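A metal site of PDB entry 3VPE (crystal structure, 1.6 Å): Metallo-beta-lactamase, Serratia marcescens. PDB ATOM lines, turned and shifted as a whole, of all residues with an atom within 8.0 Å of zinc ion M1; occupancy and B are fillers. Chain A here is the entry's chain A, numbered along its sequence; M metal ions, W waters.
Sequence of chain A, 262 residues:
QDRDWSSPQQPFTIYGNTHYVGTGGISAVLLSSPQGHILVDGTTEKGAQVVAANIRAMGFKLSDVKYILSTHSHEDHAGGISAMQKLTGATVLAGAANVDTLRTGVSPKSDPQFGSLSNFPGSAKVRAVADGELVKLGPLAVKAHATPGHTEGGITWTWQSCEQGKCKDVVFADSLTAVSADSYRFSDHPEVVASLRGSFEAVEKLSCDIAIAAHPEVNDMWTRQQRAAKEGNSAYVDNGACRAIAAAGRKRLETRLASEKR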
ATOM      1  N   TRP A   5      16.068   2.447 -24.883  1.00  0.00           N
ATOM      2  CA  TRP A   5      15.969   1.117 -24.312  1.00  0.00           C
ATOM      3  C   TRP A   5      14.658   0.448 -24.558  1.00  0.00           C
ATOM      4  O   TRP A   5      14.576  -0.790 -24.553  1.00  0.00           O
ATOM      5  CB  TRP A   5      16.225   1.184 -22.812  1.00  0.00           C
ATOM      6  CG  TRP A   5      17.636   1.542 -22.423  1.00  0.00           C
ATOM      7  CD1 TRP A   5      18.784   1.593 -23.209  1.00  0.00           C
ATOM      8  CD2 TRP A   5      18.100   1.876 -21.067  1.00  0.00           C
ATOM      9  NE1 TRP A   5      19.888   1.928 -22.461  1.00  0.00           N
ATOM     10  CE2 TRP A   5      19.540   2.123 -21.170  1.00  0.00           C
ATOM     11  CE3 TRP A   5      17.478   1.997 -19.826  1.00  0.00           C
ATOM     12  CZ2 TRP A   5      20.312   2.454 -20.060  1.00  0.00           C
ATOM     13  CZ3 TRP A   5      18.270   2.337 -18.725  1.00  0.00           C
ATOM     14  CH2 TRP A   5      19.638   2.562 -18.845  1.00  0.00           C
ATOM     15  N   GLY A  25      17.587  -0.412 -28.333  1.00  0.00           N
ATOM     16  CA  GLY A  25      18.674  -0.153 -27.417  1.00  0.00           C
ATOM     17  C   GLY A  25      19.115  -1.288 -26.483  1.00  0.00           C
ATOM     18  O   GLY A  25      20.171  -1.181 -25.878  1.00  0.00           O
ATOM     19  N   ILE A  26      18.308  -2.346 -26.374  1.00  0.00           N
ATOM     20  CA  ILE A  26      18.646  -3.460 -25.450  1.00  0.00           C
ATOM     21  C   ILE A  26      18.448  -4.789 -26.155  1.00  0.00           C
ATOM     22  O   ILE A  26      17.393  -5.061 -26.766  1.00  0.00           O
ATOM     23  CB  ILE A  26      17.768  -3.460 -24.184  1.00  0.00           C
ATOM     24  CG1 ILE A  26      17.932  -2.163 -23.377  1.00  0.00           C
ATOM     25  CG2 ILE A  26      18.092  -4.680 -23.300  1.00  0.00           C
ATOM     26  CD1 ILE A  26      19.295  -2.018 -22.725  1.00  0.00           C
ATOM     27  N   THR A  71      20.627 -12.199 -18.142  1.00  0.00           N
ATOM     28  CA  THR A  71      22.039 -11.797 -17.961  1.00  0.00           C
ATOM     29  C   THR A  71      22.219 -11.164 -16.582  1.00  0.00           C
ATOM     30  O   THR A  71      22.947 -11.698 -15.752  1.00  0.00           O
ATOM     31  CB  THR A  71      22.510 -10.804 -19.045  1.00  0.00           C
ATOM     32  OG1 THR A  71      21.586  -9.707 -19.129  1.00  0.00           O
ATOM     33  CG2 THR A  71      22.649 -11.526 -20.418  1.00  0.00           C
ATOM     34  N   HIS A  72      21.568 -10.030 -16.335  1.00  0.00           N
ATOM     35  CA  HIS A  72      21.649  -9.453 -15.003  1.00  0.00           C
ATOM     36  C   HIS A  72      20.406  -8.655 -14.681  1.00  0.00           C
ATOM     37  O   HIS A  72      19.636  -8.242 -15.568  1.00  0.00           O
ATOM     38  CB  HIS A  72      22.949  -8.642 -14.810  1.00  0.00           C
ATOM     39  CG  HIS A  72      22.990  -7.350 -15.574  1.00  0.00           C
ATOM     40  ND1 HIS A  72      23.526  -7.235 -16.793  1.00  0.00           N
ATOM     41  CD2 HIS A  72      22.584  -6.059 -15.213  1.00  0.00           C
ATOM     42  CE1 HIS A  72      23.457  -5.955 -17.224  1.00  0.00           C
ATOM     43  NE2 HIS A  72      22.868  -5.238 -16.250  1.00  0.00           N
ATOM     44  N   HIS A  74      19.162  -5.690 -13.810  1.00  0.00           N
ATOM     45  CA  HIS A  74      18.923  -4.246 -13.902  1.00  0.00           C
ATOM     46  C   HIS A  74      17.702  -4.037 -14.744  1.00  0.00           C
ATOM     47  O   HIS A  74      17.459  -4.845 -15.659  1.00  0.00           O
ATOM     48  CB  HIS A  74      20.107  -3.527 -14.502  1.00  0.00           C
ATOM     49  CG  HIS A  74      21.258  -3.381 -13.556  1.00  0.00           C
ATOM     50  ND1 HIS A  74      22.512  -3.137 -13.980  1.00  0.00           N
ATOM     51  CD2 HIS A  74      21.311  -3.426 -12.172  1.00  0.00           C
ATOM     52  CE1 HIS A  74      23.313  -3.039 -12.907  1.00  0.00           C
ATOM     53  NE2 HIS A  74      22.575  -3.220 -11.800  1.00  0.00           N
ATOM     54  N   GLU A  75      16.969  -2.957 -14.473  1.00  0.00           N
ATOM     55  CA  GLU A  75      15.714  -2.704 -15.157  1.00  0.00           C
ATOM     56  C   GLU A  75      15.798  -2.692 -16.681  1.00  0.00           C
ATOM     57  O   GLU A  75      14.807  -3.049 -17.337  1.00  0.00           O
ATOM     58  CB  GLU A  75      15.050  -1.385 -14.669  1.00  0.00           C
ATOM     59  CG  GLU A  75      15.838  -0.118 -14.967  1.00  0.00           C
ATOM     60  CD  GLU A  75      15.384   0.607 -16.239  1.00  0.00           C
ATOM     61  OE1 GLU A  75      14.450   0.127 -16.928  1.00  0.00           O
ATOM     62  OE2 GLU A  75      15.955   1.679 -16.537  1.00  0.00           O
ATOM     63  N   ASP A  76      16.934  -2.272 -17.233  1.00  0.00           N
ATOM     64  CA  ASP A  76      17.059  -2.153 -18.697  1.00  0.00           C
ATOM     65  C   ASP A  76      17.096  -3.526 -19.396  1.00  0.00           C
ATOM     66  O   ASP A  76      16.723  -3.617 -20.580  1.00  0.00           O
ATOM     67  CB  ASP A  76      18.196  -1.207 -19.155  1.00  0.00           C
ATOM     68  CG  ASP A  76      19.561  -1.548 -18.584  1.00  0.00           C
ATOM     69  OD1 ASP A  76      19.641  -2.003 -17.413  1.00  0.00           O
ATOM     70  OD2 ASP A  76      20.565  -1.288 -19.299  1.00  0.00           O
ATOM     71  N   HIS A  77      17.511  -4.565 -18.659  1.00  0.00           N
ATOM     72  CA  HIS A  77      17.547  -5.957 -19.216  1.00  0.00           C
ATOM     73  C   HIS A  77      16.473  -6.875 -18.701  1.00  0.00           C
ATOM     74  O   HIS A  77      16.044  -7.806 -19.400  1.00  0.00           O
ATOM     75  CB  HIS A  77      18.930  -6.601 -18.957  1.00  0.00           C
ATOM     76  CG  HIS A  77      20.051  -5.725 -19.408  1.00  0.00           C
ATOM     77  ND1 HIS A  77      20.505  -5.693 -20.703  1.00  0.00           N
ATOM     78  CD2 HIS A  77      20.728  -4.725 -18.719  1.00  0.00           C
ATOM     79  CE1 HIS A  77      21.482  -4.778 -20.800  1.00  0.00           C
ATOM     80  NE2 HIS A  77      21.615  -4.164 -19.592  1.00  0.00           N
ATOM     81  N   ALA A  78      16.069  -6.670 -17.433  1.00  0.00           N
ATOM     82  CA  ALA A  78      15.196  -7.557 -16.699  1.00  0.00           C
ATOM     83  C   ALA A  78      13.822  -6.919 -16.412  1.00  0.00           C
ATOM     84  O   ALA A  78      12.933  -7.645 -15.978  1.00  0.00           O
ATOM     85  CB  ALA A  78      15.859  -7.939 -15.384  1.00  0.00           C
ATOM     86  N   GLN A 113      24.462  -0.218  -9.081  1.00  0.00           N
ATOM     87  CA  GLN A 113      23.407   0.676  -9.577  1.00  0.00           C
ATOM     88  C   GLN A 113      22.162   0.587  -8.723  1.00  0.00           C
ATOM     89  O   GLN A 113      21.043   0.900  -9.174  1.00  0.00           O
ATOM     90  CB  GLN A 113      23.115   0.452 -11.073  1.00  0.00           C
ATOM     91  CG  GLN A 113      24.293   0.908 -11.912  1.00  0.00           C
ATOM     92  CD  GLN A 113      24.029   0.967 -13.394  1.00  0.00           C
ATOM     93  OE1 GLN A 113      23.397   1.880 -13.867  1.00  0.00           O
ATOM     94  NE2 GLN A 113      24.535  -0.027 -14.139  1.00  0.00           N
ATOM     95  N   LEU A 117      19.376   3.151 -10.734  1.00  0.00           N
ATOM     96  CA  LEU A 117      18.410   2.483 -11.626  1.00  0.00           C
ATOM     97  C   LEU A 117      17.164   2.132 -10.822  1.00  0.00           C
ATOM     98  O   LEU A 117      17.243   1.871  -9.630  1.00  0.00           O
ATOM     99  CB  LEU A 117      19.040   1.229 -12.271  1.00  0.00           C
ATOM    100  CG  LEU A 117      20.072   1.523 -13.367  1.00  0.00           C
ATOM    101  CD1 LEU A 117      20.526   0.230 -14.039  1.00  0.00           C
ATOM    102  CD2 LEU A 117      19.540   2.441 -14.457  1.00  0.00           C
ATOM    103  N   HIS A 150      29.492  -6.191 -12.707  1.00  0.00           N
ATOM    104  CA  HIS A 150      28.446  -5.178 -12.946  1.00  0.00           C
ATOM    105  C   HIS A 150      27.237  -5.426 -12.050  1.00  0.00           C
ATOM    106  O   HIS A 150      26.559  -4.453 -11.626  1.00  0.00           O
ATOM    107  CB  HIS A 150      28.137  -5.232 -14.456  1.00  0.00           C
ATOM    108  CG  HIS A 150      27.078  -4.287 -14.933  1.00  0.00           C
ATOM    109  ND1 HIS A 150      27.343  -3.050 -15.427  1.00  0.00           N
ATOM    110  CD2 HIS A 150      25.717  -4.482 -15.065  1.00  0.00           C
ATOM    111  CE1 HIS A 150      26.182  -2.483 -15.827  1.00  0.00           C
ATOM    112  NE2 HIS A 150      25.191  -3.339 -15.588  1.00  0.00           N
ATOM    113  N   ASP A 174      27.026 -10.776 -21.101  1.00  0.00           N
ATOM    114  CA  ASP A 174      26.551  -9.873 -20.063  1.00  0.00           C
ATOM    115  C   ASP A 174      27.440  -8.631 -20.060  1.00  0.00           C
ATOM    116  O   ASP A 174      28.573  -8.617 -20.573  1.00  0.00           O
ATOM    117  CB  ASP A 174      26.635 -10.583 -18.718  1.00  0.00           C
ATOM    118  CG  ASP A 174      25.932  -9.829 -17.604  1.00  0.00           C
ATOM    119  OD1 ASP A 174      25.038  -8.998 -17.945  1.00  0.00           O
ATOM    120  OD2 ASP A 174      26.243 -10.119 -16.430  1.00  0.00           O
ATOM    121  N   SER A 175      26.927  -7.581 -19.432  1.00  0.00           N
ATOM    122  CA  SER A 175      27.711  -6.326 -19.316  1.00  0.00           C
ATOM    123  C   SER A 175      28.871  -6.445 -18.378  1.00  0.00           C
ATOM    124  O   SER A 175      28.718  -6.996 -17.287  1.00  0.00           O
ATOM    125  CB  SER A 175      26.784  -5.245 -18.766  1.00  0.00           C
ATOM    126  OG  SER A 175      25.694  -5.062 -19.650  1.00  0.00           O
ATOM    127  N   THR A 177      30.734  -3.683 -17.546  1.00  0.00           N
ATOM    128  CA  THR A 177      31.039  -2.254 -17.308  1.00  0.00           C
ATOM    129  C   THR A 177      31.009  -1.816 -15.824  1.00  0.00           C
ATOM    130  O   THR A 177      30.036  -2.099 -15.091  1.00  0.00           O
ATOM    131  CB  THR A 177      30.026  -1.404 -18.058  1.00  0.00           C
ATOM    132  OG1 THR A 177      28.697  -1.874 -17.761  1.00  0.00           O
ATOM    133  CG2 THR A 177      30.295  -1.517 -19.572  1.00  0.00           C
ATOM    134  N   VAL A 179      30.082   0.677 -14.087  1.00  0.00           N
ATOM    135  CA  VAL A 179      29.193   1.842 -13.971  1.00  0.00           C
ATOM    136  C   VAL A 179      28.347   1.714 -12.714  1.00  0.00           C
ATOM    137  O   VAL A 179      28.146   0.604 -12.210  1.00  0.00           O
ATOM    138  CB  VAL A 179      28.341   2.002 -15.235  1.00  0.00           C
ATOM    139  CG1 VAL A 179      29.232   2.401 -16.404  1.00  0.00           C
ATOM    140  CG2 VAL A 179      27.596   0.702 -15.535  1.00  0.00           C
ATOM    141  N   ALA A 214      24.768  -7.411 -24.342  1.00  0.00           N
ATOM    142  CA  ALA A 214      23.504  -7.010 -23.729  1.00  0.00           C
ATOM    143  C   ALA A 214      23.064  -5.596 -24.168  1.00  0.00           C
ATOM    144  O   ALA A 214      21.896  -5.410 -24.444  1.00  0.00           O
ATOM    145  CB  ALA A 214      23.610  -7.150 -22.209  1.00  0.00           C
ATOM    146  N   HIS A 215      24.022  -4.655 -24.236  1.00  0.00           N
ATOM    147  CA  HIS A 215      23.823  -3.415 -24.981  1.00  0.00           C
ATOM    148  C   HIS A 215      24.390  -3.671 -26.356  1.00  0.00           C
ATOM    149  O   HIS A 215      25.607  -3.787 -26.499  1.00  0.00           O
ATOM    150  CB  HIS A 215      24.529  -2.272 -24.267  1.00  0.00           C
ATOM    151  CG  HIS A 215      23.824  -1.849 -23.012  1.00  0.00           C
ATOM    152  ND1 HIS A 215      22.869  -0.886 -23.009  1.00  0.00           N
ATOM    153  CD2 HIS A 215      23.951  -2.302 -21.704  1.00  0.00           C
ATOM    154  CE1 HIS A 215      22.356  -0.759 -21.765  1.00  0.00           C
ATOM    155  NE2 HIS A 215      23.025  -1.614 -20.945  1.00  0.00           N
HETATM  156 ZN    ZN M   1      22.395  -2.321 -19.122  1.00  0.00          ZN
HETATM  157 ZN    ZN M   2      23.221  -3.240 -15.898  1.00  0.00          ZN
HETATM  158  O   HOH W   1      22.375  -1.922 -17.101  1.00  0.00           O
HETATM  159  O   HOH W   2      24.471  -2.953 -18.685  1.00  0.00           O
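Zinc ion M1 is bound by a ring nitrogen (NE2) of His 215, a ring nitrogen (NE2) of His 77, water W1, the side-chain carboxylate (OD2) of Asp 76 and water W2.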
